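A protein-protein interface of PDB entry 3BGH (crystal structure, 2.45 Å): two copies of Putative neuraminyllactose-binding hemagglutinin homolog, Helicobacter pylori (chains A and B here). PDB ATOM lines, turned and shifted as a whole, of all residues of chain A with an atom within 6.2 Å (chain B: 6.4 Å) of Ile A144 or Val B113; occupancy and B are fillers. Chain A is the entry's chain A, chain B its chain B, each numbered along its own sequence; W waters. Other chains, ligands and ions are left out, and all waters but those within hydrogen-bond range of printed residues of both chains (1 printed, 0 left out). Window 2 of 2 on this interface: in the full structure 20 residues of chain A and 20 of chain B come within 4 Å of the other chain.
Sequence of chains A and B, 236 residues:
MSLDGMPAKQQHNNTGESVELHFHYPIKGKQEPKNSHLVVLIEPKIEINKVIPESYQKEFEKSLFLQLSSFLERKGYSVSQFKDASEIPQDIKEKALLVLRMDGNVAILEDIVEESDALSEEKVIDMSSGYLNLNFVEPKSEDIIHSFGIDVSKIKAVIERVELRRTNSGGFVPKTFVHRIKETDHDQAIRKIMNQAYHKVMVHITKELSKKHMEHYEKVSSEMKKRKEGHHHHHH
Printed residues of chain A that touch a printed residue of chain B: Asn A135, Ile A144, Ile A145, His A146 and Ser A147.
Of the 10 printed residues of chain B, 4 touch a printed residue of chain A.
Hydrophobic or aromatic side chains of chain B within 4 Å of the printed part of chain A: Ile B112 and Val B113.
Among the printed residues, 6 pairs touch across the chains.
Among the printed residues, no Asp or Glu carboxylate lies within 4 Å of a Lys or Arg side-chain nitrogen of the other chain.
Water W1 bridges O of Val B113 (2.7 Å) and N of Ser A147 (3.0 Å).
Among the printed residues, pairs that only touch across the chains: Ile A144 with Val B113, Ile A145 with Glu B115 and Ser A147 with Ile B112.
O of Asp B111 lies within hydrogen-bond range of ND2 of Asn A135 (3.0 Å).
A ring nitrogen (ND1) of His A146 is in hydrogen-bond range of the side-chain carboxylate of Glu B115, 2.5 Å away.
The side-chain hydroxyl (OG) of Ser A147 is in hydrogen-bond range of the backbone NH (N) of Val B113 (2.8 Å).
OD1 of Asn A135 sits at hydrogen-bond distance from ND2 of Asn A133.
OG of Ser A147 sits at hydrogen-bond distance from OD1 of Asn A135, 2.7 Å away.
The backbone carbonyl oxygen (O) of Phe A136 is in hydrogen-bond range of the backbone NH (N) of Ile A145 (2.7 Å).
The backbone carbonyl oxygen of His A146 sits at hydrogen-bond distance from the backbone NH of Phe A136 (2.8 Å).
N of Asp B111 sits at hydrogen-bond distance from O of Ile B125 (3.2 Å).
The backbone carbonyl oxygen (O) of Ile B112 lies within hydrogen-bond range of the backbone NH (N) of Ile B125, at 2.8 Å.
Printed residues of chain B within 4 Å of Asn A135: Asp B111 (3.0 Å).
Of the printed residues of chain B, Ile A144 touches Val B113 (3.5 Å).
Printed residues of chain B within 4 Å of His A146: Glu B115.
Printed residues of chain A within 4 Å of Asp B111: Asn A135 (3.0 Å).
Of the printed residues of chain A, Ile B112 touches Ser A147.
Of chain A, only Ile A144 (3.5 Å) and Ser A147 (2.8 Å) come within 4 Å of Val B113.
Glu B122 touches none of the printed residues of chain A.
The nearest printed residue of chain B that does not touch Ile A144 is Asp B111 (4.01 Å).
The nearest residue of chain A that does not touch Val B113 is Ile A145 (4.5 Å).
The nearest printed residue of chain B that does not touch Asn A135 is Ile B112 (4.8 Å).
No position is printed for both chains.
Of the 6 pairs that touch across the chains among the printed residues, none has its exchanged pair printed and touching as well.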
ATOM      1  N   ASN A 133      27.369 -26.844  13.054  1.00  0.00           N
ATOM      2  CA  ASN A 133      26.119 -26.613  12.399  1.00  0.00           C
ATOM      3  C   ASN A 133      26.063 -25.283  11.673  1.00  0.00           C
ATOM      4  O   ASN A 133      26.128 -24.213  12.297  1.00  0.00           O
ATOM      5  CB  ASN A 133      24.999 -26.654  13.408  1.00  0.00           C
ATOM      6  CG  ASN A 133      23.672 -26.753  12.749  1.00  0.00           C
ATOM      7  OD1 ASN A 133      23.338 -27.792  12.138  1.00  0.00           O
ATOM      8  ND2 ASN A 133      22.894 -25.684  12.834  1.00  0.00           N
ATOM      9  N   ASN A 135      23.614 -22.787  10.002  1.00  0.00           N
ATOM     10  CA  ASN A 135      22.194 -22.395   9.852  1.00  0.00           C
ATOM     11  C   ASN A 135      21.908 -21.444   8.686  1.00  0.00           C
ATOM     12  O   ASN A 135      22.614 -20.458   8.485  1.00  0.00           O
ATOM     13  CB  ASN A 135      21.591 -21.861  11.175  1.00  0.00           C
ATOM     14  CG  ASN A 135      20.948 -22.974  12.031  1.00  0.00           C
ATOM     15  OD1 ASN A 135      20.930 -24.134  11.639  1.00  0.00           O
ATOM     16  ND2 ASN A 135      20.387 -22.609  13.178  1.00  0.00           N
ATOM     17  N   PHE A 136      20.879 -21.754   7.909  1.00  0.00           N
ATOM     18  CA  PHE A 136      20.434 -20.897   6.823  1.00  0.00           C
ATOM     19  C   PHE A 136      19.212 -20.135   7.306  1.00  0.00           C
ATOM     20  O   PHE A 136      18.182 -20.727   7.608  1.00  0.00           O
ATOM     21  CB  PHE A 136      20.081 -21.716   5.558  1.00  0.00           C
ATOM     22  CG  PHE A 136      21.243 -22.433   4.929  1.00  0.00           C
ATOM     23  CD1 PHE A 136      21.615 -22.151   3.626  1.00  0.00           C
ATOM     24  CD2 PHE A 136      21.938 -23.425   5.615  1.00  0.00           C
ATOM     25  CE1 PHE A 136      22.673 -22.844   3.023  1.00  0.00           C
ATOM     26  CE2 PHE A 136      23.020 -24.109   5.011  1.00  0.00           C
ATOM     27  CZ  PHE A 136      23.389 -23.813   3.737  1.00  0.00           C
ATOM     28  N   VAL A 137      19.331 -18.817   7.381  1.00  0.00           N
ATOM     29  CA  VAL A 137      18.322 -17.985   8.016  1.00  0.00           C
ATOM     30  C   VAL A 137      17.747 -16.940   7.057  1.00  0.00           C
ATOM     31  O   VAL A 137      18.485 -16.245   6.341  1.00  0.00           O
ATOM     32  CB  VAL A 137      18.880 -17.286   9.283  1.00  0.00           C
ATOM     33  CG1 VAL A 137      17.786 -16.507   9.997  1.00  0.00           C
ATOM     34  CG2 VAL A 137      19.519 -18.285  10.247  1.00  0.00           C
ATOM     35  N   GLU A 138      16.418 -16.856   7.051  1.00  0.00           N
ATOM     36  CA  GLU A 138      15.678 -15.810   6.343  1.00  0.00           C
ATOM     37  C   GLU A 138      15.788 -14.485   7.117  1.00  0.00           C
ATOM     38  O   GLU A 138      15.383 -14.394   8.266  1.00  0.00           O
ATOM     39  CB  GLU A 138      14.245 -16.269   6.015  1.00  0.00           C
ATOM     40  CG  GLU A 138      13.096 -15.315   6.334  1.00  0.00           C
ATOM     41  CD  GLU A 138      13.181 -13.950   5.636  1.00  0.00           C
ATOM     42  OE1 GLU A 138      13.595 -13.894   4.457  1.00  0.00           O
ATOM     43  OE2 GLU A 138      12.820 -12.937   6.287  1.00  0.00           O
ATOM     44  N   GLU A 142      14.075 -13.754  10.654  1.00  0.00           N
ATOM     45  CA  GLU A 142      15.046 -14.503  11.473  1.00  0.00           C
ATOM     46  C   GLU A 142      14.746 -16.019  11.575  1.00  0.00           C
ATOM     47  O   GLU A 142      15.311 -16.711  12.405  1.00  0.00           O
ATOM     48  CB  GLU A 142      15.189 -13.864  12.864  1.00  0.00           C
ATOM     49  CG  GLU A 142      16.285 -12.786  12.952  1.00  0.00           C
ATOM     50  CD  GLU A 142      16.597 -12.344  14.393  1.00  0.00           C
ATOM     51  OE1 GLU A 142      15.652 -12.270  15.222  1.00  0.00           O
ATOM     52  OE2 GLU A 142      17.789 -12.062  14.691  1.00  0.00           O
ATOM     53  N   ASP A 143      13.856 -16.516  10.726  1.00  0.00           N
ATOM     54  CA  ASP A 143      13.484 -17.919  10.710  1.00  0.00           C
ATOM     55  C   ASP A 143      14.615 -18.794  10.184  1.00  0.00           C
ATOM     56  O   ASP A 143      15.229 -18.485   9.161  1.00  0.00           O
ATOM     57  CB  ASP A 143      12.309 -18.125   9.775  1.00  0.00           C
ATOM     58  CG  ASP A 143      11.025 -17.584  10.331  1.00  0.00           C
ATOM     59  OD1 ASP A 143      11.056 -16.961  11.410  1.00  0.00           O
ATOM     60  OD2 ASP A 143       9.980 -17.809   9.685  1.00  0.00           O
ATOM     61  N   ILE A 144      14.885 -19.892  10.872  1.00  0.00           N
ATOM     62  CA  ILE A 144      15.861 -20.835  10.371  1.00  0.00           C
ATOM     63  C   ILE A 144      15.139 -21.659   9.329  1.00  0.00           C
ATOM     64  O   ILE A 144      14.071 -22.184   9.613  1.00  0.00           O
ATOM     65  CB  ILE A 144      16.452 -21.714  11.498  1.00  0.00           C
ATOM     66  CG1 ILE A 144      17.190 -20.829  12.522  1.00  0.00           C
ATOM     67  CG2 ILE A 144      17.394 -22.765  10.909  1.00  0.00           C
ATOM     68  CD1 ILE A 144      17.097 -21.317  13.950  1.00  0.00           C
ATOM     69  N   ILE A 145      15.699 -21.728   8.121  1.00  0.00           N
ATOM     70  CA  ILE A 145      15.087 -22.458   7.016  1.00  0.00           C
ATOM     71  C   ILE A 145      15.763 -23.829   6.812  1.00  0.00           C
ATOM     72  O   ILE A 145      15.126 -24.805   6.401  1.00  0.00           O
ATOM     73  CB  ILE A 145      15.088 -21.598   5.714  1.00  0.00           C
ATOM     74  CG1 ILE A 145      13.834 -20.729   5.649  1.00  0.00           C
ATOM     75  CG2 ILE A 145      15.067 -22.443   4.439  1.00  0.00           C
ATOM     76  CD1 ILE A 145      13.900 -19.483   6.467  1.00  0.00           C
ATOM     77  N   HIS A 146      17.048 -23.921   7.115  1.00  0.00           N
ATOM     78  CA  HIS A 146      17.756 -25.132   6.822  1.00  0.00           C
ATOM     79  C   HIS A 146      18.991 -25.231   7.673  1.00  0.00           C
ATOM     80  O   HIS A 146      19.646 -24.217   7.903  1.00  0.00           O
ATOM     81  CB  HIS A 146      18.143 -25.140   5.348  1.00  0.00           C
ATOM     82  CG  HIS A 146      18.766 -26.417   4.928  1.00  0.00           C
ATOM     83  ND1 HIS A 146      18.026 -27.558   4.713  1.00  0.00           N
ATOM     84  CD2 HIS A 146      20.061 -26.768   4.768  1.00  0.00           C
ATOM     85  CE1 HIS A 146      18.836 -28.544   4.366  1.00  0.00           C
ATOM     86  NE2 HIS A 146      20.075 -28.094   4.411  1.00  0.00           N
ATOM     87  N   SER A 147      19.314 -26.440   8.128  1.00  0.00           N
ATOM     88  CA  SER A 147      20.491 -26.674   8.950  1.00  0.00           C
ATOM     89  C   SER A 147      21.354 -27.710   8.269  1.00  0.00           C
ATOM     90  O   SER A 147      20.855 -28.761   7.898  1.00  0.00           O
ATOM     91  CB  SER A 147      20.110 -27.194  10.350  1.00  0.00           C
ATOM     92  OG  SER A 147      19.353 -26.243  11.083  1.00  0.00           O
ATOM     93  N   ASP B 111      19.026 -25.215  18.463  1.00  0.00           N
ATOM     94  CA  ASP B 111      18.286 -24.637  17.316  1.00  0.00           C
ATOM     95  C   ASP B 111      18.702 -25.233  15.976  1.00  0.00           C
ATOM     96  O   ASP B 111      19.204 -24.528  15.104  1.00  0.00           O
ATOM     97  CB  ASP B 111      18.376 -23.106  17.310  1.00  0.00           C
ATOM     98  CG  ASP B 111      17.709 -22.474  18.553  1.00  0.00           C
ATOM     99  OD1 ASP B 111      16.632 -22.975  18.981  1.00  0.00           O
ATOM    100  OD2 ASP B 111      18.257 -21.511  19.135  1.00  0.00           O
ATOM    101  N   ILE B 112      18.501 -26.540  15.827  1.00  0.00           N
ATOM    102  CA  ILE B 112      18.788 -27.227  14.584  1.00  0.00           C
ATOM    103  C   ILE B 112      17.438 -27.505  13.969  1.00  0.00           C
ATOM    104  O   ILE B 112      16.525 -27.936  14.663  1.00  0.00           O
ATOM    105  CB  ILE B 112      19.584 -28.546  14.827  1.00  0.00           C
ATOM    106  CG1 ILE B 112      20.960 -28.225  15.423  1.00  0.00           C
ATOM    107  CG2 ILE B 112      19.708 -29.376  13.539  1.00  0.00           C
ATOM    108  CD1 ILE B 112      21.834 -29.436  15.620  1.00  0.00           C
ATOM    109  N   VAL B 113      17.285 -27.218  12.684  1.00  0.00           N
ATOM    110  CA  VAL B 113      16.032 -27.527  12.032  1.00  0.00           C
ATOM    111  C   VAL B 113      16.130 -28.847  11.294  1.00  0.00           C
ATOM    112  O   VAL B 113      17.143 -29.165  10.670  1.00  0.00           O
ATOM    113  CB  VAL B 113      15.517 -26.374  11.108  1.00  0.00           C
ATOM    114  CG1 VAL B 113      14.294 -26.807  10.301  1.00  0.00           C
ATOM    115  CG2 VAL B 113      15.102 -25.193  11.950  1.00  0.00           C
ATOM    116  N   GLU B 114      15.067 -29.630  11.435  1.00  0.00           N
ATOM    117  CA  GLU B 114      14.830 -30.802  10.619  1.00  0.00           C
ATOM    118  C   GLU B 114      13.559 -30.496   9.857  1.00  0.00           C
ATOM    119  O   GLU B 114      12.524 -30.164  10.438  1.00  0.00           O
ATOM    120  CB  GLU B 114      14.722 -32.060  11.491  1.00  0.00           C
ATOM    121  CG  GLU B 114      15.978 -32.219  12.395  1.00  0.00           C
ATOM    122  CD  GLU B 114      16.182 -33.627  12.986  1.00  0.00           C
ATOM    123  OE1 GLU B 114      15.183 -34.275  13.412  1.00  0.00           O
ATOM    124  OE2 GLU B 114      17.372 -34.039  13.062  1.00  0.00           O
ATOM    125  N   GLU B 115      13.660 -30.545   8.546  1.00  0.00           N
ATOM    126  CA  GLU B 115      12.583 -30.146   7.707  1.00  0.00           C
ATOM    127  C   GLU B 115      11.536 -31.251   7.612  1.00  0.00           C
ATOM    128  O   GLU B 115      11.807 -32.405   7.880  1.00  0.00           O
ATOM    129  CB  GLU B 115      13.143 -29.766   6.338  1.00  0.00           C
ATOM    130  CG  GLU B 115      13.871 -28.432   6.361  1.00  0.00           C
ATOM    131  CD  GLU B 115      14.284 -27.971   4.988  1.00  0.00           C
ATOM    132  OE1 GLU B 115      15.509 -27.964   4.708  1.00  0.00           O
ATOM    133  OE2 GLU B 115      13.374 -27.624   4.200  1.00  0.00           O
ATOM    134  N   GLU B 122       8.072 -30.565  10.456  1.00  0.00           N
ATOM    135  CA  GLU B 122       9.225 -29.719  10.712  1.00  0.00           C
ATOM    136  C   GLU B 122       9.431 -29.478  12.210  1.00  0.00           C
ATOM    137  O   GLU B 122       8.483 -29.208  12.935  1.00  0.00           O
ATOM    138  CB  GLU B 122       9.082 -28.366  10.009  1.00  0.00           C
ATOM    139  CG  GLU B 122      10.305 -27.420  10.203  1.00  0.00           C
ATOM    140  CD  GLU B 122      10.187 -26.081   9.492  1.00  0.00           C
ATOM    141  OE1 GLU B 122      10.709 -25.103  10.040  1.00  0.00           O
ATOM    142  OE2 GLU B 122       9.566 -25.976   8.397  1.00  0.00           O
ATOM    143  N   LYS B 123      10.685 -29.553  12.652  1.00  0.00           N
ATOM    144  CA  LYS B 123      11.036 -29.502  14.068  1.00  0.00           C
ATOM    145  C   LYS B 123      12.297 -28.699  14.277  1.00  0.00           C
ATOM    146  O   LYS B 123      13.207 -28.768  13.469  1.00  0.00           O
ATOM    147  CB  LYS B 123      11.338 -30.896  14.578  1.00  0.00           C
ATOM    148  CG  LYS B 123      10.197 -31.837  14.662  1.00  0.00           C
ATOM    149  CD  LYS B 123      10.677 -33.140  15.265  1.00  0.00           C
ATOM    150  CE  LYS B 123      10.894 -34.200  14.213  1.00  0.00           C
ATOM    151  NZ  LYS B 123       9.545 -34.682  13.795  1.00  0.00           N
ATOM    152  N   VAL B 124      12.347 -27.962  15.381  1.00  0.00           N
ATOM    153  CA  VAL B 124      13.564 -27.361  15.892  1.00  0.00           C
ATOM    154  C   VAL B 124      14.002 -28.237  17.082  1.00  0.00           C
ATOM    155  O   VAL B 124      13.185 -28.559  17.940  1.00  0.00           O
ATOM    156  CB  VAL B 124      13.314 -25.915  16.361  1.00  0.00           C
ATOM    157  CG1 VAL B 124      14.619 -25.271  16.855  1.00  0.00           C
ATOM    158  CG2 VAL B 124      12.687 -25.097  15.242  1.00  0.00           C
ATOM    159  N   ILE B 125      15.284 -28.612  17.124  1.00  0.00           N
ATOM    160  CA  ILE B 125      15.778 -29.528  18.149  1.00  0.00           C
ATOM    161  C   ILE B 125      17.056 -28.991  18.783  1.00  0.00           C
ATOM    162  O   ILE B 125      17.725 -28.105  18.205  1.00  0.00           O
ATOM    163  CB  ILE B 125      16.090 -30.977  17.586  1.00  0.00           C
ATOM    164  CG1 ILE B 125      17.340 -30.930  16.688  1.00  0.00           C
ATOM    165  CG2 ILE B 125      14.854 -31.606  16.914  1.00  0.00           C
ATOM    166  CD1 ILE B 125      17.771 -32.255  16.075  1.00  0.00           C
ATOM    167  N   ARG B 180       2.942 -23.140  14.574  1.00  0.00           N
ATOM    168  CA  ARG B 180       4.101 -23.600  15.316  1.00  0.00           C
ATOM    169  C   ARG B 180       3.811 -23.746  16.838  1.00  0.00           C
ATOM    170  O   ARG B 180       3.098 -22.944  17.440  1.00  0.00           O
ATOM    171  CB  ARG B 180       5.381 -22.838  14.933  1.00  0.00           C
ATOM    172  CG  ARG B 180       5.954 -21.868  15.933  1.00  0.00           C
ATOM    173  CD  ARG B 180       7.103 -21.064  15.281  1.00  0.00           C
ATOM    174  NE  ARG B 180       8.294 -21.880  15.053  1.00  0.00           N
ATOM    175  CZ  ARG B 180       8.908 -22.046  13.882  1.00  0.00           C
ATOM    176  NH1 ARG B 180       9.984 -22.824  13.804  1.00  0.00           N
ATOM    177  NH2 ARG B 180       8.461 -21.438  12.789  1.00  0.00           N
HETATM  178  O   HOH W   1      17.430 -28.756   8.012  1.00  0.00           O
